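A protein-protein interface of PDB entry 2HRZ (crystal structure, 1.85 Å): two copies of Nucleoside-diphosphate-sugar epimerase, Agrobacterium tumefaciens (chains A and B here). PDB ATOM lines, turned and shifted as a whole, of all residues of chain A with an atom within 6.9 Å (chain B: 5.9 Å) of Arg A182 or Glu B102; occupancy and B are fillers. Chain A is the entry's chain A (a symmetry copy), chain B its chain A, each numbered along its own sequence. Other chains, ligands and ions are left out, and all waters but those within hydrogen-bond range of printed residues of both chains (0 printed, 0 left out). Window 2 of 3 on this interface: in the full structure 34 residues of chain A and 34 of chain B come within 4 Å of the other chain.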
ATOM      1  N   ARG A 124     -10.431  17.741 -14.452  1.00  0.00           N
ATOM      2  CA  ARG A 124      -9.635  18.958 -14.589  1.00  0.00           C
ATOM      3  C   ARG A 124      -9.264  19.210 -16.060  1.00  0.00           C
ATOM      4  O   ARG A 124      -9.419  20.324 -16.571  1.00  0.00           O
ATOM      5  CB  ARG A 124      -8.388  18.855 -13.709  1.00  0.00           C
ATOM      6  CG  ARG A 124      -7.390  19.982 -13.896  1.00  0.00           C
ATOM      7  CD  ARG A 124      -6.194  19.755 -12.983  1.00  0.00           C
ATOM      8  NE  ARG A 124      -5.423  18.598 -13.422  1.00  0.00           N
ATOM      9  CZ  ARG A 124      -4.467  18.645 -14.340  1.00  0.00           C
ATOM     10  NH1 ARG A 124      -4.135  19.803 -14.908  1.00  0.00           N
ATOM     11  NH2 ARG A 124      -3.840  17.536 -14.693  1.00  0.00           N
ATOM     12  N   ASN A 127     -12.220  20.264 -17.975  1.00  0.00           N
ATOM     13  CA  ASN A 127     -12.567  21.645 -17.622  1.00  0.00           C
ATOM     14  C   ASN A 127     -11.724  22.638 -18.437  1.00  0.00           C
ATOM     15  O   ASN A 127     -12.229  23.644 -18.944  1.00  0.00           O
ATOM     16  CB  ASN A 127     -12.373  21.907 -16.131  1.00  0.00           C
ATOM     17  CG  ASN A 127     -12.656  23.349 -15.762  1.00  0.00           C
ATOM     18  OD1 ASN A 127     -11.725  24.147 -15.622  1.00  0.00           O
ATOM     19  ND2 ASN A 127     -13.948  23.708 -15.656  1.00  0.00           N
ATOM     20  N   LYS A 133     -17.712  21.371 -15.877  1.00  0.00           N
ATOM     21  CA  LYS A 133     -17.590  21.654 -14.447  1.00  0.00           C
ATOM     22  C   LYS A 133     -18.722  20.966 -13.678  1.00  0.00           C
ATOM     23  O   LYS A 133     -19.703  21.603 -13.305  1.00  0.00           O
ATOM     24  CB  LYS A 133     -17.577  23.169 -14.188  1.00  0.00           C
ATOM     25  CG  LYS A 133     -17.227  23.562 -12.743  1.00  0.00           C
ATOM     26  CD  LYS A 133     -17.130  25.095 -12.610  1.00  0.00           C
ATOM     27  CE  LYS A 133     -16.825  25.529 -11.199  1.00  0.00           C
ATOM     28  NZ  LYS A 133     -16.985  27.010 -11.089  1.00  0.00           N
ATOM     29  N   SER A 177     -11.109  19.611  -2.121  1.00  0.00           N
ATOM     30  CA  SER A 177     -11.175  21.050  -1.816  1.00  0.00           C
ATOM     31  C   SER A 177     -10.298  21.884  -2.757  1.00  0.00           C
ATOM     32  O   SER A 177     -10.700  22.986  -3.159  1.00  0.00           O
ATOM     33  CB  SER A 177     -10.828  21.347  -0.360  1.00  0.00           C
ATOM     34  OG  SER A 177     -11.821  20.847   0.516  1.00  0.00           O
ATOM     35  N   ASP A 178      -9.095  21.395  -3.077  1.00  0.00           N
ATOM     36  CA  ASP A 178      -8.172  22.173  -3.927  1.00  0.00           C
ATOM     37  C   ASP A 178      -8.652  22.277  -5.379  1.00  0.00           C
ATOM     38  O   ASP A 178      -8.611  23.358  -5.980  1.00  0.00           O
ATOM     39  CB  ASP A 178      -6.740  21.619  -3.879  1.00  0.00           C
ATOM     40  CG  ASP A 178      -5.716  22.624  -4.370  1.00  0.00           C
ATOM     41  OD1 ASP A 178      -5.737  23.785  -3.903  1.00  0.00           O
ATOM     42  OD2 ASP A 178      -4.887  22.253  -5.227  1.00  0.00           O
ATOM     43  N   TYR A 179      -9.102  21.155  -5.943  1.00  0.00           N
ATOM     44  CA  TYR A 179      -9.659  21.168  -7.310  1.00  0.00           C
ATOM     45  C   TYR A 179     -10.920  22.020  -7.411  1.00  0.00           C
ATOM     46  O   TYR A 179     -11.148  22.692  -8.431  1.00  0.00           O
ATOM     47  CB  TYR A 179      -9.963  19.748  -7.775  1.00  0.00           C
ATOM     48  CG  TYR A 179      -8.736  18.956  -8.201  1.00  0.00           C
ATOM     49  CD1 TYR A 179      -7.637  18.781  -7.330  1.00  0.00           C
ATOM     50  CD2 TYR A 179      -8.685  18.349  -9.460  1.00  0.00           C
ATOM     51  CE1 TYR A 179      -6.501  18.022  -7.728  1.00  0.00           C
ATOM     52  CE2 TYR A 179      -7.584  17.593  -9.859  1.00  0.00           C
ATOM     53  CZ  TYR A 179      -6.491  17.435  -8.992  1.00  0.00           C
ATOM     54  OH  TYR A 179      -5.405  16.680  -9.410  1.00  0.00           O
ATOM     55  N   SER A 180     -11.747  21.975  -6.368  1.00  0.00           N
ATOM     56  CA  SER A 180     -12.947  22.826  -6.287  1.00  0.00           C
ATOM     57  C   SER A 180     -12.582  24.301  -6.255  1.00  0.00           C
ATOM     58  O   SER A 180     -13.178  25.105  -6.968  1.00  0.00           O
ATOM     59  CB  SER A 180     -13.791  22.485  -5.046  1.00  0.00           C
ATOM     60  OG  SER A 180     -14.354  21.174  -5.146  1.00  0.00           O
ATOM     61  N   ARG A 181     -11.602  24.654  -5.424  1.00  0.00           N
ATOM     62  CA  ARG A 181     -11.140  26.044  -5.303  1.00  0.00           C
ATOM     63  C   ARG A 181     -10.620  26.570  -6.649  1.00  0.00           C
ATOM     64  O   ARG A 181     -10.857  27.726  -7.012  1.00  0.00           O
ATOM     65  CB  ARG A 181     -10.027  26.139  -4.249  1.00  0.00           C
ATOM     66  CG  ARG A 181      -9.496  27.569  -3.976  1.00  0.00           C
ATOM     67  CD  ARG A 181      -8.322  27.556  -2.982  1.00  0.00           C
ATOM     68  NE  ARG A 181      -7.159  26.810  -3.492  1.00  0.00           N
ATOM     69  CZ  ARG A 181      -6.272  27.290  -4.361  1.00  0.00           C
ATOM     70  NH1 ARG A 181      -6.391  28.533  -4.826  1.00  0.00           N
ATOM     71  NH2 ARG A 181      -5.254  26.538  -4.760  1.00  0.00           N
ATOM     72  N   ARG A 182      -9.905  25.714  -7.375  1.00  0.00           N
ATOM     73  CA  ARG A 182      -9.287  26.108  -8.647  1.00  0.00           C
ATOM     74  C   ARG A 182     -10.310  26.070  -9.790  1.00  0.00           C
ATOM     75  O   ARG A 182      -9.996  26.397 -10.950  1.00  0.00           O
ATOM     76  CB  ARG A 182      -8.039  25.268  -8.932  1.00  0.00           C
ATOM     77  CG  ARG A 182      -6.895  25.516  -7.901  1.00  0.00           C
ATOM     78  CD  ARG A 182      -5.586  24.798  -8.267  1.00  0.00           C
ATOM     79  NE  ARG A 182      -4.958  25.455  -9.413  1.00  0.00           N
ATOM     80  CZ  ARG A 182      -3.709  25.908  -9.464  1.00  0.00           C
ATOM     81  NH1 ARG A 182      -2.869  25.750  -8.444  1.00  0.00           N
ATOM     82  NH2 ARG A 182      -3.292  26.500 -10.577  1.00  0.00           N
ATOM     83  N   GLY A 183     -11.533  25.684  -9.441  1.00  0.00           N
ATOM     84  CA  GLY A 183     -12.686  25.768 -10.341  1.00  0.00           C
ATOM     85  C   GLY A 183     -12.830  24.664 -11.380  1.00  0.00           C
ATOM     86  O   GLY A 183     -13.498  24.858 -12.397  1.00  0.00           O
ATOM     87  N   PHE A 184     -12.234  23.499 -11.126  1.00  0.00           N
ATOM     88  CA  PHE A 184     -12.317  22.379 -12.062  1.00  0.00           C
ATOM     89  C   PHE A 184     -13.638  21.624 -11.959  1.00  0.00           C
ATOM     90  O   PHE A 184     -14.118  21.085 -12.945  1.00  0.00           O
ATOM     91  CB  PHE A 184     -11.142  21.402 -11.876  1.00  0.00           C
ATOM     92  CG  PHE A 184      -9.792  22.054 -11.949  1.00  0.00           C
ATOM     93  CD1 PHE A 184      -9.496  22.967 -12.964  1.00  0.00           C
ATOM     94  CD2 PHE A 184      -8.795  21.730 -11.004  1.00  0.00           C
ATOM     95  CE1 PHE A 184      -8.232  23.566 -13.038  1.00  0.00           C
ATOM     96  CE2 PHE A 184      -7.538  22.327 -11.067  1.00  0.00           C
ATOM     97  CZ  PHE A 184      -7.259  23.251 -12.083  1.00  0.00           C
ATOM     98  N   PHE A 185     -14.187  21.559 -10.746  1.00  0.00           N
ATOM     99  CA  PHE A 185     -15.518  21.001 -10.502  1.00  0.00           C
ATOM    100  C   PHE A 185     -16.090  21.560  -9.210  1.00  0.00           C
ATOM    101  O   PHE A 185     -15.379  22.220  -8.454  1.00  0.00           O
ATOM    102  CB  PHE A 185     -15.515  19.454 -10.495  1.00  0.00           C
ATOM    103  CG  PHE A 185     -14.505  18.806  -9.545  1.00  0.00           C
ATOM    104  CD1 PHE A 185     -14.795  18.623  -8.188  1.00  0.00           C
ATOM    105  CD2 PHE A 185     -13.312  18.283 -10.049  1.00  0.00           C
ATOM    106  CE1 PHE A 185     -13.898  17.969  -7.328  1.00  0.00           C
ATOM    107  CE2 PHE A 185     -12.402  17.624  -9.204  1.00  0.00           C
ATOM    108  CZ  PHE A 185     -12.695  17.472  -7.832  1.00  0.00           C
ATOM    109  N   VAL B  97       8.111  26.442  -4.643  1.00  0.00           N
ATOM    110  CA  VAL B  97       7.440  27.387  -3.772  1.00  0.00           C
ATOM    111  C   VAL B  97       6.002  27.638  -4.222  1.00  0.00           C
ATOM    112  O   VAL B  97       5.648  27.404  -5.388  1.00  0.00           O
ATOM    113  CB  VAL B  97       8.230  28.716  -3.634  1.00  0.00           C
ATOM    114  CG1 VAL B  97       9.632  28.445  -3.032  1.00  0.00           C
ATOM    115  CG2 VAL B  97       8.338  29.452  -4.984  1.00  0.00           C
ATOM    116  N   SER B  98       5.192  28.097  -3.277  1.00  0.00           N
ATOM    117  CA  SER B  98       3.758  28.281  -3.460  1.00  0.00           C
ATOM    118  C   SER B  98       3.414  29.149  -4.679  1.00  0.00           C
ATOM    119  O   SER B  98       2.471  28.849  -5.431  1.00  0.00           O
ATOM    120  CB  SER B  98       3.172  28.904  -2.192  1.00  0.00           C
ATOM    121  OG  SER B  98       1.762  28.974  -2.271  1.00  0.00           O
ATOM    122  N   GLY B  99       4.172  30.229  -4.873  1.00  0.00           N
ATOM    123  CA  GLY B  99       3.891  31.138  -5.985  1.00  0.00           C
ATOM    124  C   GLY B  99       3.950  30.405  -7.312  1.00  0.00           C
ATOM    125  O   GLY B  99       3.116  30.611  -8.200  1.00  0.00           O
ATOM    126  N   GLU B 100       4.941  29.539  -7.433  1.00  0.00           N
ATOM    127  CA  GLU B 100       5.130  28.732  -8.619  1.00  0.00           C
ATOM    128  C   GLU B 100       4.064  27.641  -8.728  1.00  0.00           C
ATOM    129  O   GLU B 100       3.494  27.421  -9.795  1.00  0.00           O
ATOM    130  CB  GLU B 100       6.508  28.104  -8.568  1.00  0.00           C
ATOM    131  CG  GLU B 100       7.160  28.027  -9.910  1.00  0.00           C
ATOM    132  CD  GLU B 100       8.611  27.654  -9.777  1.00  0.00           C
ATOM    133  OE1 GLU B 100       9.403  28.502  -9.299  1.00  0.00           O
ATOM    134  OE2 GLU B 100       8.948  26.506 -10.127  1.00  0.00           O
ATOM    135  N   ALA B 101       3.817  26.947  -7.616  1.00  0.00           N
ATOM    136  CA  ALA B 101       2.793  25.900  -7.571  1.00  0.00           C
ATOM    137  C   ALA B 101       1.405  26.435  -7.926  1.00  0.00           C
ATOM    138  O   ALA B 101       0.609  25.732  -8.561  1.00  0.00           O
ATOM    139  CB  ALA B 101       2.773  25.224  -6.194  1.00  0.00           C
ATOM    140  N   GLU B 102       1.103  27.664  -7.512  1.00  0.00           N
ATOM    141  CA  GLU B 102      -0.209  28.236  -7.802  1.00  0.00           C
ATOM    142  C   GLU B 102      -0.373  28.534  -9.302  1.00  0.00           C
ATOM    143  O   GLU B 102      -1.439  28.269  -9.874  1.00  0.00           O
ATOM    144  CB  GLU B 102      -0.473  29.472  -6.949  1.00  0.00           C
ATOM    145  CG  GLU B 102      -1.954  29.725  -6.627  1.00  0.00           C
ATOM    146  CD  GLU B 102      -2.725  28.527  -6.021  1.00  0.00           C
ATOM    147  OE1 GLU B 102      -2.162  27.693  -5.266  1.00  0.00           O
ATOM    148  OE2 GLU B 102      -3.932  28.431  -6.318  1.00  0.00           O
ATOM    149  N   LEU B 103       0.685  29.043  -9.939  1.00  0.00           N
ATOM    150  CA  LEU B 103       0.641  29.379 -11.364  1.00  0.00           C
ATOM    151  C   LEU B 103       0.812  28.179 -12.297  1.00  0.00           C
ATOM    152  O   LEU B 103       0.411  28.233 -13.474  1.00  0.00           O
ATOM    153  CB  LEU B 103       1.659  30.479 -11.694  1.00  0.00           C
ATOM    154  CG  LEU B 103       1.283  31.882 -11.186  1.00  0.00           C
ATOM    155  CD1 LEU B 103       2.399  32.896 -11.403  1.00  0.00           C
ATOM    156  CD2 LEU B 103      -0.036  32.409 -11.794  1.00  0.00           C
ATOM    157  N   ASP B 104       1.409  27.103 -11.788  1.00  0.00           N
ATOM    158  CA  ASP B 104       1.673  25.927 -12.595  1.00  0.00           C
ATOM    159  C   ASP B 104       1.117  24.716 -11.858  1.00  0.00           C
ATOM    160  O   ASP B 104       1.841  24.073 -11.093  1.00  0.00           O
ATOM    161  CB  ASP B 104       3.185  25.776 -12.845  1.00  0.00           C
ATOM    162  CG  ASP B 104       3.506  24.773 -13.942  1.00  0.00           C
ATOM    163  OD1 ASP B 104       2.755  23.792 -14.127  1.00  0.00           O
ATOM    164  OD2 ASP B 104       4.538  24.961 -14.630  1.00  0.00           O
ATOM    165  N   PHE B 105      -0.168  24.436 -12.070  1.00  0.00           N
ATOM    166  CA  PHE B 105      -0.838  23.341 -11.366  1.00  0.00           C
ATOM    167  C   PHE B 105      -0.042  22.036 -11.459  1.00  0.00           C
ATOM    168  O   PHE B 105       0.211  21.386 -10.436  1.00  0.00           O
ATOM    169  CB  PHE B 105      -2.266  23.135 -11.884  1.00  0.00           C
ATOM    170  CG  PHE B 105      -2.962  21.968 -11.254  1.00  0.00           C
ATOM    171  CD1 PHE B 105      -3.796  22.150 -10.164  1.00  0.00           C
ATOM    172  CD2 PHE B 105      -2.761  20.677 -11.742  1.00  0.00           C
ATOM    173  CE1 PHE B 105      -4.440  21.044  -9.565  1.00  0.00           C
ATOM    174  CE2 PHE B 105      -3.378  19.584 -11.144  1.00  0.00           C
ATOM    175  CZ  PHE B 105      -4.231  19.775 -10.056  1.00  0.00           C
ATOM    176  N   TYR B 109       2.036  19.850  -8.263  1.00  0.00           N
ATOM    177  CA  TYR B 109       1.637  18.496  -7.865  1.00  0.00           C
ATOM    178  C   TYR B 109       2.712  17.466  -8.157  1.00  0.00           C
ATOM    179  O   TYR B 109       2.913  16.552  -7.372  1.00  0.00           O
ATOM    180  CB  TYR B 109       0.296  18.082  -8.470  1.00  0.00           C
ATOM    181  CG  TYR B 109      -0.850  18.556  -7.605  1.00  0.00           C
ATOM    182  CD1 TYR B 109      -1.490  19.768  -7.858  1.00  0.00           C
ATOM    183  CD2 TYR B 109      -1.245  17.812  -6.492  1.00  0.00           C
ATOM    184  CE1 TYR B 109      -2.542  20.231  -7.009  1.00  0.00           C
ATOM    185  CE2 TYR B 109      -2.274  18.235  -5.667  1.00  0.00           C
ATOM    186  CZ  TYR B 109      -2.910  19.446  -5.913  1.00  0.00           C
ATOM    187  OH  TYR B 109      -3.924  19.822  -5.069  1.00  0.00           O
ATOM    188  N   LEU B 162      -5.731  26.855   1.564  1.00  0.00           N
ATOM    189  CA  LEU B 162      -6.307  27.535   0.416  1.00  0.00           C
ATOM    190  C   LEU B 162      -5.306  27.775  -0.734  1.00  0.00           C
ATOM    191  O   LEU B 162      -5.535  28.619  -1.592  1.00  0.00           O
ATOM    192  CB  LEU B 162      -7.026  28.824   0.866  1.00  0.00           C
ATOM    193  CG  LEU B 162      -8.164  28.619   1.882  1.00  0.00           C
ATOM    194  CD1 LEU B 162      -8.619  29.943   2.524  1.00  0.00           C
ATOM    195  CD2 LEU B 162      -9.350  27.910   1.232  1.00  0.00           C
ATOM    196  N   THR B 163      -4.209  27.007  -0.744  1.00  0.00           N
ATOM    197  CA  THR B 163      -3.251  26.990  -1.848  1.00  0.00           C
ATOM    198  C   THR B 163      -2.991  25.541  -2.250  1.00  0.00           C
ATOM    199  O   THR B 163      -3.194  24.637  -1.438  1.00  0.00           O
ATOM    200  CB  THR B 163      -1.889  27.628  -1.470  1.00  0.00           C
ATOM    201  OG1 THR B 163      -1.269  26.883  -0.415  1.00  0.00           O
ATOM    202  CG2 THR B 163      -2.069  29.094  -1.016  1.00  0.00           C
ATOM    203  N   SER B 164      -2.538  25.327  -3.480  1.00  0.00           N
ATOM    204  CA  SER B 164      -2.119  23.989  -3.898  1.00  0.00           C
ATOM    205  C   SER B 164      -0.889  23.528  -3.120  1.00  0.00           C
ATOM    206  O   SER B 164      -0.783  22.362  -2.763  1.00  0.00           O
ATOM    207  CB  SER B 164      -1.893  23.937  -5.412  1.00  0.00           C
ATOM    208  OG  SER B 164      -3.115  24.261  -6.076  1.00  0.00           O
ATOM    209  N   TYR B 165       0.027  24.459  -2.845  1.00  0.00           N
ATOM    210  CA  TYR B 165       1.209  24.154  -2.047  1.00  0.00           C
ATOM    211  C   TYR B 165       0.809  23.602  -0.668  1.00  0.00           C
ATOM    212  O   TYR B 165       1.332  22.593  -0.234  1.00  0.00           O
ATOM    213  CB  TYR B 165       2.041  25.415  -1.876  1.00  0.00           C
ATOM    214  CG  TYR B 165       3.307  25.230  -1.067  1.00  0.00           C
ATOM    215  CD1 TYR B 165       4.522  24.962  -1.698  1.00  0.00           C
ATOM    216  CD2 TYR B 165       3.295  25.366   0.316  1.00  0.00           C
ATOM    217  CE1 TYR B 165       5.699  24.807  -0.961  1.00  0.00           C
ATOM    218  CE2 TYR B 165       4.462  25.213   1.065  1.00  0.00           C
ATOM    219  CZ  TYR B 165       5.653  24.936   0.419  1.00  0.00           C
ATOM    220  OH  TYR B 165       6.817  24.798   1.151  1.00  0.00           O
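No position is printed for both chains.
Of the 14 pairs that touch across the chains among the printed residues, none has its exchanged pair printed and touching as well.
The side-chain hydroxyl of Ser B164 sits at hydrogen-bond distance from the side-chain carboxylate of Asp A178 (2.8 Å).
NH1 of Arg A182 lies within hydrogen-bond range of OG of Ser B164, 2.8 Å away.
The guanidinium group (NH1) of Arg A182 is in hydrogen-bond range of the backbone carbonyl oxygen (O) of Ala B101 (3.5 Å).
The side-chain carboxylate of Glu B102 lies within salt-bridge range of the guanidinium group of Arg A181 (2.8 Å).
NE of Arg A181 sits at hydrogen-bond distance from O of Leu B162, at 3.1 Å.
The guanidinium group (NH1) of Arg A182 lies within salt-bridge range of the side-chain carboxylate (OE2) of Glu B102 (3.6 Å).
The side-chain hydroxyl of Tyr B109 sits at hydrogen-bond distance from the side-chain carboxylate of Asp A178.
OG of Ser B164 sits at hydrogen-bond distance from NH2 of Arg A181 (3.4 Å).
Of the 12 printed residues of chain A, 6 touch a printed residue of chain B.
Printed residues of chain A that touch a printed residue of chain B: Arg A124, Asp A178, Tyr A179, Arg A181, Arg A182 and Phe A184.
Hydrophobic or aromatic side chains of chain A that line the printed part of chain B: Tyr A179 and Phe A184.
Hydrophobic or aromatic side chains of chain B that line the printed part of chain A: Phe B105 and Tyr B109.
Along chain B the printed residues that touch a printed residue of chain A span positions 101 to 164.
Among the printed residues, 14 pairs touch across the chains.
Among the printed residues, Asp or Glu carboxylates within 4 Å of a Lys or Arg side-chain nitrogen of the other chain: Arg A181 with Glu B102 (2.8 Å) and Arg A182 with Glu B102 (3.6 Å).
Arg A182 touches just these residues of chain B: Ala B101 (3.5 Å), Glu B102 (2.7 Å), Phe B105 (3.6 Å) and Ser B164 (2.8 Å).
Of the printed residues of chain B, Arg A124 touches Phe B105.
Of the printed residues of chain B, Tyr A179 touches Phe B105 (3.4 Å).
Of the printed residues of chain A, Ser B164 touches Asp A178, Arg A181 and Arg A182.
Glu B100 touches none of the printed residues of chain A.
Lys A133 touches none of the printed residues of chain B.
The nearest residue of chain B that does not touch Arg A182 is Leu B103 (4.8 Å).
NH2 of Arg A181 is in salt-bridge range of OD1 of Asp A178.
The side-chain carboxylate (OE1) of Glu B102 sits at hydrogen-bond distance from the backbone NH (N) of Ser B164, 3.0 Å away.
N of Phe A184 lies within hydrogen-bond range of O of Tyr A179 (3.0 Å).
Among the printed residues, pairs that only touch across the chains: Arg A124 with Phe B105 (3.2 Å), Tyr A179 with Phe B105 (3.4 Å), Arg A181 with Thr B163 (3.5 Å), Arg A182 with Phe B105 (3.6 Å), Asp A178 with Thr B163 (3.6 Å) and Phe A184 with Phe B105 (3.7 Å).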
